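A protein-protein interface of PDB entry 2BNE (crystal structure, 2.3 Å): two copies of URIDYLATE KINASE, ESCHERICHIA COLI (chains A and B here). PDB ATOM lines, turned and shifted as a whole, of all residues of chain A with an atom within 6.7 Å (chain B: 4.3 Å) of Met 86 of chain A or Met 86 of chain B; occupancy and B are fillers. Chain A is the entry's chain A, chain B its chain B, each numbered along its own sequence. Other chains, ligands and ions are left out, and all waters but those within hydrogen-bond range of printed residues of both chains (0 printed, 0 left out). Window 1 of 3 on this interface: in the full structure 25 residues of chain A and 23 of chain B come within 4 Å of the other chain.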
ATOM      1  N   ILE A  29      -6.075 -20.974 -18.669  1.00  0.00           N
ATOM      2  CA  ILE A  29      -7.491 -20.945 -18.994  1.00  0.00           C
ATOM      3  C   ILE A  29      -7.925 -22.272 -19.594  1.00  0.00           C
ATOM      4  O   ILE A  29      -7.225 -22.838 -20.428  1.00  0.00           O
ATOM      5  CB  ILE A  29      -7.794 -19.816 -19.991  1.00  0.00           C
ATOM      6  CG1 ILE A  29      -7.402 -18.471 -19.370  1.00  0.00           C
ATOM      7  CG2 ILE A  29      -9.264 -19.834 -20.368  1.00  0.00           C
ATOM      8  CD1 ILE A  29      -7.484 -17.291 -20.322  1.00  0.00           C
ATOM      9  N   ILE A  55     -14.616  -9.765 -15.167  1.00  0.00           N
ATOM     10  CA  ILE A  55     -13.835 -10.971 -15.015  1.00  0.00           C
ATOM     11  C   ILE A  55     -12.564 -10.808 -14.183  1.00  0.00           C
ATOM     12  O   ILE A  55     -11.911  -9.769 -14.209  1.00  0.00           O
ATOM     13  CB  ILE A  55     -13.512 -11.541 -16.413  1.00  0.00           C
ATOM     14  CG1 ILE A  55     -12.815 -12.884 -16.281  1.00  0.00           C
ATOM     15  CG2 ILE A  55     -12.678 -10.542 -17.207  1.00  0.00           C
ATOM     16  CD1 ILE A  55     -12.988 -13.739 -17.518  1.00  0.00           C
ATOM     17  N   LEU A  60      -4.155 -16.249 -13.219  1.00  0.00           N
ATOM     18  CA  LEU A  60      -2.906 -15.983 -13.910  1.00  0.00           C
ATOM     19  C   LEU A  60      -1.976 -15.203 -12.977  1.00  0.00           C
ATOM     20  O   LEU A  60      -0.894 -15.676 -12.647  1.00  0.00           O
ATOM     21  CB  LEU A  60      -3.180 -15.193 -15.192  1.00  0.00           C
ATOM     22  CG  LEU A  60      -4.335 -15.755 -16.033  1.00  0.00           C
ATOM     23  CD1 LEU A  60      -4.632 -14.843 -17.232  1.00  0.00           C
ATOM     24  CD2 LEU A  60      -3.979 -17.150 -16.510  1.00  0.00           C
ATOM     25  N   PHE A  61      -2.400 -14.021 -12.535  1.00  0.00           N
ATOM     26  CA  PHE A  61      -1.564 -13.219 -11.650  1.00  0.00           C
ATOM     27  C   PHE A  61      -2.334 -12.436 -10.591  1.00  0.00           C
ATOM     28  O   PHE A  61      -3.420 -11.930 -10.843  1.00  0.00           O
ATOM     29  CB  PHE A  61      -0.722 -12.212 -12.451  1.00  0.00           C
ATOM     30  CG  PHE A  61       0.324 -12.835 -13.324  1.00  0.00           C
ATOM     31  CD1 PHE A  61       0.138 -12.913 -14.701  1.00  0.00           C
ATOM     32  CD2 PHE A  61       1.508 -13.318 -12.776  1.00  0.00           C
ATOM     33  CE1 PHE A  61       1.122 -13.463 -15.528  1.00  0.00           C
ATOM     34  CE2 PHE A  61       2.497 -13.871 -13.596  1.00  0.00           C
ATOM     35  CZ  PHE A  61       2.300 -13.940 -14.974  1.00  0.00           C
ATOM     36  N   MET A  71       8.373  -7.967  -6.266  1.00  0.00           N
ATOM     37  CA  MET A  71       7.985  -6.976  -7.266  1.00  0.00           C
ATOM     38  C   MET A  71       7.265  -5.770  -6.669  1.00  0.00           C
ATOM     39  O   MET A  71       6.626  -5.871  -5.622  1.00  0.00           O
ATOM     40  CB  MET A  71       7.089  -7.643  -8.300  1.00  0.00           C
ATOM     41  CG  MET A  71       6.768  -6.799  -9.498  1.00  0.00           C
ATOM     42  SD  MET A  71       5.661  -7.686 -10.599  1.00  0.00           S
ATOM     43  CE  MET A  71       6.742  -8.932 -11.223  1.00  0.00           C
ATOM     44  N   VAL A  75       3.225  -2.478 -10.089  1.00  0.00           N
ATOM     45  CA  VAL A  75       3.481  -3.227 -11.312  1.00  0.00           C
ATOM     46  C   VAL A  75       2.822  -4.606 -11.221  1.00  0.00           C
ATOM     47  O   VAL A  75       2.357  -5.155 -12.223  1.00  0.00           O
ATOM     48  CB  VAL A  75       4.996  -3.404 -11.566  1.00  0.00           C
ATOM     49  CG1 VAL A  75       5.211  -4.170 -12.853  1.00  0.00           C
ATOM     50  CG2 VAL A  75       5.672  -2.039 -11.634  1.00  0.00           C
ATOM     51  N   HIS A  78      -0.697  -4.099 -12.045  1.00  0.00           N
ATOM     52  CA  HIS A  78      -0.883  -3.833 -13.469  1.00  0.00           C
ATOM     53  C   HIS A  78      -0.876  -5.167 -14.202  1.00  0.00           C
ATOM     54  O   HIS A  78      -1.642  -5.378 -15.144  1.00  0.00           O
ATOM     55  CB  HIS A  78       0.228  -2.942 -14.019  1.00  0.00           C
ATOM     56  CG  HIS A  78       0.121  -1.516 -13.587  1.00  0.00           C
ATOM     57  ND1 HIS A  78       1.042  -0.558 -13.954  1.00  0.00           N
ATOM     58  CD2 HIS A  78      -0.802  -0.880 -12.827  1.00  0.00           C
ATOM     59  CE1 HIS A  78       0.688   0.607 -13.440  1.00  0.00           C
ATOM     60  NE2 HIS A  78      -0.427   0.438 -12.753  1.00  0.00           N
ATOM     61  N   MET A  79      -0.013  -6.075 -13.769  1.00  0.00           N
ATOM     62  CA  MET A  79       0.038  -7.369 -14.415  1.00  0.00           C
ATOM     63  C   MET A  79      -1.277  -8.079 -14.142  1.00  0.00           C
ATOM     64  O   MET A  79      -1.863  -8.682 -15.038  1.00  0.00           O
ATOM     65  CB  MET A  79       1.228  -8.171 -13.888  1.00  0.00           C
ATOM     66  CG  MET A  79       2.563  -7.728 -14.496  1.00  0.00           C
ATOM     67  SD  MET A  79       3.997  -8.438 -13.650  1.00  0.00           S
ATOM     68  CE  MET A  79       3.861 -10.159 -14.219  1.00  0.00           C
ATOM     69  N   GLY A  80      -1.756  -7.974 -12.906  1.00  0.00           N
ATOM     70  CA  GLY A  80      -3.012  -8.614 -12.542  1.00  0.00           C
ATOM     71  C   GLY A  80      -4.136  -8.094 -13.411  1.00  0.00           C
ATOM     72  O   GLY A  80      -4.945  -8.859 -13.924  1.00  0.00           O
ATOM     73  N   MET A  81      -4.193  -6.780 -13.579  1.00  0.00           N
ATOM     74  CA  MET A  81      -5.236  -6.208 -14.414  1.00  0.00           C
ATOM     75  C   MET A  81      -5.093  -6.722 -15.842  1.00  0.00           C
ATOM     76  O   MET A  81      -6.088  -7.086 -16.466  1.00  0.00           O
ATOM     77  CB  MET A  81      -5.182  -4.683 -14.361  1.00  0.00           C
ATOM     78  CG  MET A  81      -5.697  -4.138 -13.039  1.00  0.00           C
ATOM     79  SD  MET A  81      -5.847  -2.350 -12.997  1.00  0.00           S
ATOM     80  CE  MET A  81      -4.206  -1.901 -12.418  1.00  0.00           C
ATOM     81  N   LEU A  82      -3.862  -6.779 -16.349  1.00  0.00           N
ATOM     82  CA  LEU A  82      -3.648  -7.286 -17.694  1.00  0.00           C
ATOM     83  C   LEU A  82      -4.172  -8.707 -17.803  1.00  0.00           C
ATOM     84  O   LEU A  82      -4.730  -9.090 -18.824  1.00  0.00           O
ATOM     85  CB  LEU A  82      -2.165  -7.280 -18.067  1.00  0.00           C
ATOM     86  CG  LEU A  82      -1.562  -5.950 -18.508  1.00  0.00           C
ATOM     87  CD1 LEU A  82      -0.145  -6.202 -19.035  1.00  0.00           C
ATOM     88  CD2 LEU A  82      -2.441  -5.306 -19.584  1.00  0.00           C
ATOM     89  N   ALA A  83      -3.974  -9.484 -16.740  1.00  0.00           N
ATOM     90  CA  ALA A  83      -4.428 -10.860 -16.717  1.00  0.00           C
ATOM     91  C   ALA A  83      -5.942 -10.908 -16.926  1.00  0.00           C
ATOM     92  O   ALA A  83      -6.448 -11.799 -17.616  1.00  0.00           O
ATOM     93  CB  ALA A  83      -4.050 -11.513 -15.398  1.00  0.00           C
ATOM     94  N   THR A  84      -6.665  -9.947 -16.354  1.00  0.00           N
ATOM     95  CA  THR A  84      -8.113  -9.943 -16.524  1.00  0.00           C
ATOM     96  C   THR A  84      -8.464  -9.652 -17.979  1.00  0.00           C
ATOM     97  O   THR A  84      -9.486 -10.116 -18.477  1.00  0.00           O
ATOM     98  CB  THR A  84      -8.812  -8.896 -15.633  1.00  0.00           C
ATOM     99  OG1 THR A  84      -8.558  -7.585 -16.142  1.00  0.00           O
ATOM    100  CG2 THR A  84      -8.326  -9.002 -14.204  1.00  0.00           C
ATOM    101  N   VAL A  85      -7.619  -8.890 -18.667  1.00  0.00           N
ATOM    102  CA  VAL A  85      -7.881  -8.590 -20.072  1.00  0.00           C
ATOM    103  C   VAL A  85      -7.695  -9.872 -20.878  1.00  0.00           C
ATOM    104  O   VAL A  85      -8.422 -10.122 -21.838  1.00  0.00           O
ATOM    105  CB  VAL A  85      -6.947  -7.475 -20.589  1.00  0.00           C
ATOM    106  CG1 VAL A  85      -7.132  -7.261 -22.085  1.00  0.00           C
ATOM    107  CG2 VAL A  85      -7.259  -6.187 -19.849  1.00  0.00           C
ATOM    108  N   MET A  86      -6.734 -10.696 -20.470  1.00  0.00           N
ATOM    109  CA  MET A  86      -6.478 -11.956 -21.158  1.00  0.00           C
ATOM    110  C   MET A  86      -7.690 -12.864 -21.013  1.00  0.00           C
ATOM    111  O   MET A  86      -8.103 -13.503 -21.973  1.00  0.00           O
ATOM    112  CB  MET A  86      -5.231 -12.632 -20.592  1.00  0.00           C
ATOM    113  CG  MET A  86      -4.001 -11.762 -20.740  1.00  0.00           C
ATOM    114  SD  MET A  86      -2.457 -12.572 -20.294  1.00  0.00           S
ATOM    115  CE  MET A  86      -1.942 -13.126 -21.936  1.00  0.00           C
ATOM    116  N   ASN A  87      -8.266 -12.908 -19.812  1.00  0.00           N
ATOM    117  CA  ASN A  87      -9.449 -13.726 -19.575  1.00  0.00           C
ATOM    118  C   ASN A  87     -10.620 -13.120 -20.340  1.00  0.00           C
ATOM    119  O   ASN A  87     -11.391 -13.828 -20.976  1.00  0.00           O
ATOM    120  CB  ASN A  87      -9.783 -13.795 -18.076  1.00  0.00           C
ATOM    121  CG  ASN A  87      -8.812 -14.677 -17.295  1.00  0.00           C
ATOM    122  OD1 ASN A  87      -8.310 -15.681 -17.810  1.00  0.00           O
ATOM    123  ND2 ASN A  87      -8.564 -14.316 -16.037  1.00  0.00           N
ATOM    124  N   GLY A  88     -10.749 -11.799 -20.281  1.00  0.00           N
ATOM    125  CA  GLY A  88     -11.826 -11.142 -21.000  1.00  0.00           C
ATOM    126  C   GLY A  88     -11.755 -11.473 -22.480  1.00  0.00           C
ATOM    127  O   GLY A  88     -12.776 -11.682 -23.141  1.00  0.00           O
ATOM    128  N   LEU A  89     -10.536 -11.520 -22.996  1.00  0.00           N
ATOM    129  CA  LEU A  89     -10.284 -11.827 -24.399  1.00  0.00           C
ATOM    130  C   LEU A  89     -10.773 -13.239 -24.722  1.00  0.00           C
ATOM    131  O   LEU A  89     -11.507 -13.452 -25.687  1.00  0.00           O
ATOM    132  CB  LEU A  89      -8.782 -11.718 -24.657  1.00  0.00           C
ATOM    133  CG  LEU A  89      -8.240 -10.863 -25.801  1.00  0.00           C
ATOM    134  CD1 LEU A  89      -9.052  -9.603 -25.955  1.00  0.00           C
ATOM    135  CD2 LEU A  89      -6.773 -10.538 -25.514  1.00  0.00           C
ATOM    136  N   ALA A  90     -10.362 -14.205 -23.904  1.00  0.00           N
ATOM    137  CA  ALA A  90     -10.758 -15.590 -24.115  1.00  0.00           C
ATOM    138  C   ALA A  90     -12.270 -15.763 -23.953  1.00  0.00           C
ATOM    139  O   ALA A  90     -12.898 -16.516 -24.694  1.00  0.00           O
ATOM    140  CB  ALA A  90     -10.010 -16.508 -23.134  1.00  0.00           C
ATOM    141  N   MET A  91     -12.850 -15.076 -22.975  1.00  0.00           N
ATOM    142  CA  MET A  91     -14.282 -15.189 -22.741  1.00  0.00           C
ATOM    143  C   MET A  91     -15.054 -14.583 -23.918  1.00  0.00           C
ATOM    144  O   MET A  91     -16.017 -15.173 -24.409  1.00  0.00           O
ATOM    145  CB  MET A  91     -14.664 -14.489 -21.427  1.00  0.00           C
ATOM    146  CG  MET A  91     -16.144 -14.563 -21.070  1.00  0.00           C
ATOM    147  SD  MET A  91     -16.799 -16.257 -21.008  1.00  0.00           S
ATOM    148  CE  MET A  91     -15.952 -16.862 -19.553  1.00  0.00           C
ATOM    149  N   LEU A 104     -15.682  -6.508 -25.632  1.00  0.00           N
ATOM    150  CA  LEU A 104     -14.762  -6.491 -24.505  1.00  0.00           C
ATOM    151  C   LEU A 104     -14.290  -5.065 -24.308  1.00  0.00           C
ATOM    152  O   LEU A 104     -13.785  -4.449 -25.234  1.00  0.00           O
ATOM    153  CB  LEU A 104     -13.539  -7.375 -24.762  1.00  0.00           C
ATOM    154  CG  LEU A 104     -12.420  -7.281 -23.709  1.00  0.00           C
ATOM    155  CD1 LEU A 104     -12.917  -7.719 -22.338  1.00  0.00           C
ATOM    156  CD2 LEU A 104     -11.265  -8.162 -24.134  1.00  0.00           C
ATOM    157  N   SER A 135     -12.987  -5.549 -18.384  1.00  0.00           N
ATOM    158  CA  SER A 135     -11.710  -6.066 -17.915  1.00  0.00           C
ATOM    159  C   SER A 135     -10.818  -4.973 -17.310  1.00  0.00           C
ATOM    160  O   SER A 135     -11.087  -3.775 -17.470  1.00  0.00           O
ATOM    161  CB  SER A 135     -10.990  -6.752 -19.064  1.00  0.00           C
ATOM    162  OG  SER A 135     -10.809  -5.846 -20.134  1.00  0.00           O
ATOM    163  N   LEU B  60       3.363 -18.184 -20.870  1.00  0.00           N
ATOM    164  CA  LEU B  60       2.008 -17.888 -20.436  1.00  0.00           C
ATOM    165  C   LEU B  60       1.017 -18.351 -21.505  1.00  0.00           C
ATOM    166  O   LEU B  60       0.194 -19.216 -21.253  1.00  0.00           O
ATOM    167  CB  LEU B  60       1.866 -16.383 -20.171  1.00  0.00           C
ATOM    168  CG  LEU B  60       3.003 -15.781 -19.329  1.00  0.00           C
ATOM    169  CD1 LEU B  60       2.834 -14.270 -19.200  1.00  0.00           C
ATOM    170  CD2 LEU B  60       3.018 -16.422 -17.953  1.00  0.00           C
ATOM    171  N   PHE B  61       1.101 -17.785 -22.701  1.00  0.00           N
ATOM    172  CA  PHE B  61       0.197 -18.183 -23.772  1.00  0.00           C
ATOM    173  C   PHE B  61       0.847 -18.206 -25.147  1.00  0.00           C
ATOM    174  O   PHE B  61       1.681 -17.363 -25.455  1.00  0.00           O
ATOM    175  CB  PHE B  61      -1.011 -17.250 -23.841  1.00  0.00           C
ATOM    176  CG  PHE B  61      -1.914 -17.331 -22.653  1.00  0.00           C
ATOM    177  CD1 PHE B  61      -1.893 -16.339 -21.678  1.00  0.00           C
ATOM    178  CD2 PHE B  61      -2.809 -18.387 -22.518  1.00  0.00           C
ATOM    179  CE1 PHE B  61      -2.753 -16.390 -20.584  1.00  0.00           C
ATOM    180  CE2 PHE B  61      -3.674 -18.450 -21.427  1.00  0.00           C
ATOM    181  CZ  PHE B  61      -3.645 -17.444 -20.459  1.00  0.00           C
ATOM    182  N   MET B  79      -3.707 -12.694 -27.256  1.00  0.00           N
ATOM    183  CA  MET B  79      -3.448 -13.054 -25.876  1.00  0.00           C
ATOM    184  C   MET B  79      -1.942 -13.281 -25.730  1.00  0.00           C
ATOM    185  O   MET B  79      -1.325 -12.804 -24.787  1.00  0.00           O
ATOM    186  CB  MET B  79      -4.241 -14.305 -25.495  1.00  0.00           C
ATOM    187  CG  MET B  79      -5.721 -14.015 -25.231  1.00  0.00           C
ATOM    188  SD  MET B  79      -6.721 -15.513 -25.093  1.00  0.00           S
ATOM    189  CE  MET B  79      -6.138 -16.121 -23.517  1.00  0.00           C
ATOM    190  N   LEU B  82      -0.197 -10.116 -25.483  1.00  0.00           N
ATOM    191  CA  LEU B  82      -0.423  -9.511 -24.174  1.00  0.00           C
ATOM    192  C   LEU B  82       0.477 -10.172 -23.142  1.00  0.00           C
ATOM    193  O   LEU B  82       0.971  -9.526 -22.218  1.00  0.00           O
ATOM    194  CB  LEU B  82      -1.872  -9.671 -23.726  1.00  0.00           C
ATOM    195  CG  LEU B  82      -2.904  -8.718 -24.317  1.00  0.00           C
ATOM    196  CD1 LEU B  82      -4.234  -8.928 -23.585  1.00  0.00           C
ATOM    197  CD2 LEU B  82      -2.426  -7.274 -24.173  1.00  0.00           C
ATOM    198  N   ALA B  83       0.678 -11.471 -23.300  1.00  0.00           N
ATOM    199  CA  ALA B  83       1.523 -12.211 -22.389  1.00  0.00           C
ATOM    200  C   ALA B  83       2.940 -11.633 -22.419  1.00  0.00           C
ATOM    201  O   ALA B  83       3.608 -11.586 -21.383  1.00  0.00           O
ATOM    202  CB  ALA B  83       1.538 -13.687 -22.779  1.00  0.00           C
ATOM    203  N   THR B  84       3.401 -11.191 -23.594  1.00  0.00           N
ATOM    204  CA  THR B  84       4.750 -10.635 -23.675  1.00  0.00           C
ATOM    205  C   THR B  84       4.794  -9.302 -22.927  1.00  0.00           C
ATOM    206  O   THR B  84       5.824  -8.921 -22.372  1.00  0.00           O
ATOM    207  CB  THR B  84       5.225 -10.410 -25.133  1.00  0.00           C
ATOM    208  OG1 THR B  84       4.508  -9.310 -25.718  1.00  0.00           O
ATOM    209  CG2 THR B  84       5.019 -11.670 -25.964  1.00  0.00           C
ATOM    210  N   VAL B  85       3.676  -8.589 -22.908  1.00  0.00           N
ATOM    211  CA  VAL B  85       3.629  -7.322 -22.196  1.00  0.00           C
ATOM    212  C   VAL B  85       3.711  -7.598 -20.704  1.00  0.00           C
ATOM    213  O   VAL B  85       4.286  -6.816 -19.951  1.00  0.00           O
ATOM    214  CB  VAL B  85       2.338  -6.540 -22.510  1.00  0.00           C
ATOM    215  CG1 VAL B  85       2.244  -5.286 -21.641  1.00  0.00           C
ATOM    216  CG2 VAL B  85       2.338  -6.155 -23.983  1.00  0.00           C
ATOM    217  N   MET B  86       3.152  -8.727 -20.282  1.00  0.00           N
ATOM    218  CA  MET B  86       3.183  -9.088 -18.866  1.00  0.00           C
ATOM    219  C   MET B  86       4.613  -9.395 -18.463  1.00  0.00           C
ATOM    220  O   MET B  86       5.055  -8.987 -17.396  1.00  0.00           O
ATOM    221  CB  MET B  86       2.278 -10.289 -18.597  1.00  0.00           C
ATOM    222  CG  MET B  86       0.834  -9.996 -18.948  1.00  0.00           C
ATOM    223  SD  MET B  86      -0.348 -11.255 -18.460  1.00  0.00           S
ATOM    224  CE  MET B  86      -0.834 -10.617 -16.875  1.00  0.00           C
ATOM    225  N   ASN B  87       5.336 -10.104 -19.327  1.00  0.00           N
ATOM    226  CA  ASN B  87       6.729 -10.423 -19.053  1.00  0.00           C
ATOM    227  C   ASN B  87       7.556  -9.137 -19.117  1.00  0.00           C
ATOM    228  O   ASN B  87       8.412  -8.903 -18.275  1.00  0.00           O
ATOM    229  CB  ASN B  87       7.268 -11.440 -20.064  1.00  0.00           C
ATOM    230  CG  ASN B  87       6.734 -12.849 -19.831  1.00  0.00           C
ATOM    231  OD1 ASN B  87       6.477 -13.249 -18.694  1.00  0.00           O
ATOM    232  ND2 ASN B  87       6.597 -13.616 -20.908  1.00  0.00           N
ATOM    233  N   GLY B  88       7.284  -8.301 -20.114  1.00  0.00           N
ATOM    234  CA  GLY B  88       8.008  -7.055 -20.246  1.00  0.00           C
ATOM    235  C   GLY B  88       7.825  -6.200 -19.005  1.00  0.00           C
ATOM    236  O   GLY B  88       8.730  -5.505 -18.569  1.00  0.00           O
ATOM    237  N   LEU B  89       6.630  -6.250 -18.439  1.00  0.00           N
ATOM    238  CA  LEU B  89       6.299  -5.503 -17.228  1.00  0.00           C
ATOM    239  C   LEU B  89       7.146  -6.022 -16.051  1.00  0.00           C
ATOM    240  O   LEU B  89       7.767  -5.244 -15.311  1.00  0.00           O
ATOM    241  CB  LEU B  89       4.820  -5.707 -16.919  1.00  0.00           C
ATOM    242  CG  LEU B  89       3.883  -4.523 -16.694  1.00  0.00           C
ATOM    243  CD1 LEU B  89       4.241  -3.347 -17.580  1.00  0.00           C
ATOM    244  CD2 LEU B  89       2.455  -4.997 -16.971  1.00  0.00           C
ATOM    245  N   ALA B  90       7.160  -7.341 -15.876  1.00  0.00           N
ATOM    246  CA  ALA B  90       7.931  -7.948 -14.800  1.00  0.00           C
ATOM    247  C   ALA B  90       9.426  -7.691 -14.994  1.00  0.00           C
ATOM    248  O   ALA B  90      10.129  -7.379 -14.050  1.00  0.00           O
ATOM    249  CB  ALA B  90       7.658  -9.446 -14.738  1.00  0.00           C
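The side-chain sulfur (SD) of Met 86 of chain A lies close to the side-chain sulfur (SD) of Met 86 of chain B, 3.1 Å away.
Among the printed residues, merely in contact across the chains: Met 79 of chain A with Met 86 of chain B (2.9 Å), Met 86 of chain A with Met 79 of chain B (2.9 Å), Met 86 of chain A with Phe 61 of chain B (3.2 Å), Phe 61 of chain A with Met 86 of chain B (3.3 Å), Ala 83 of chain A with Met 86 of chain B (3.3 Å), Met 86 of chain A with Ala 83 of chain B (3.4 Å), Leu 82 of chain A with Leu 89 of chain B (3.5 Å), Leu 89 of chain A with Leu 82 of chain B (3.6 Å), Leu 89 of chain A with Met 79 of chain B (3.6 Å), Leu 82 of chain A with Val 85 of chain B (3.7 Å), Ile 29 of chain A with Met 79 of chain B (3.7 Å), Val 85 of chain A with Leu 82 of chain B (3.7 Å), Met 71 of chain A with Ala 90 of chain B (3.7 Å), Met 79 of chain A with Leu 89 of chain B (3.7 Å), Val 75 of chain A with Leu 89 of chain B (3.7 Å), Leu 82 of chain A with Met 86 of chain B (3.8 Å), Ile 29 of chain A with Phe 61 of chain B (3.8 Å), Met 86 of chain A with Leu 82 of chain B (3.9 Å), Met 79 of chain A with Ala 90 of chain B (3.9 Å), Ala 90 of chain A with Met 79 of chain B (3.9 Å), Phe 61 of chain A with Leu 60 of chain B (3.9 Å) and Leu 60 of chain A with Phe 61 of chain B (3.97 Å).
Of the 22 printed residues of chain A, 12 touch a printed residue of chain B. Printed residues of chain A that touch a printed residue of chain B: Ile 29, Leu 60, Phe 61, Met 71, Val 75, Met 79, Leu 82, Ala 83, Val 85, Met 86, Leu 89 and Ala 90. Along chain A the printed residues that touch a printed residue of chain B span positions 29 to 90. Among the printed residues, no Asp or Glu carboxylate lies within 4 Å of a Lys or Arg side-chain nitrogen of the other chain.
Leu 60 of chain A touches Phe 61 of chain B, and with the chains exchanged Phe 61 of chain A touches Leu 60 of chain B. Met 79 of chain A touches Met 86 of chain B, and with the chains exchanged Met 86 of chain A touches Met 79 of chain B. Met 79 of chain A touches Leu 89 of chain B, and with the chains exchanged Leu 89 of chain A touches Met 79 of chain B. Leu 82 of chain A touches Val 85 of chain B, and with the chains exchanged Val 85 of chain A touches Leu 82 of chain B. 12 positions are printed for both chains. Of the 23 pairs that touch across the chains among the printed residues, 19 have their exchanged pair printed and touching as well.
Of the printed residues of chain B, Leu 60 of chain A touches Phe 61 (3.97 Å). Of the printed residues of chain B, Ala 83 of chain A touches Met 86. Of chain A, only Phe 61, Met 79, Leu 82, Ala 83 and Met 86 come within 4 Å of Met 86 of chain B. The nearest printed residue of chain B that does not touch Met 86 of chain A is Leu 60 of chain B (5.3 Å). The nearest residue of chain A that does not touch Met 86 of chain B is Gly 80 of chain A (4.9 Å).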
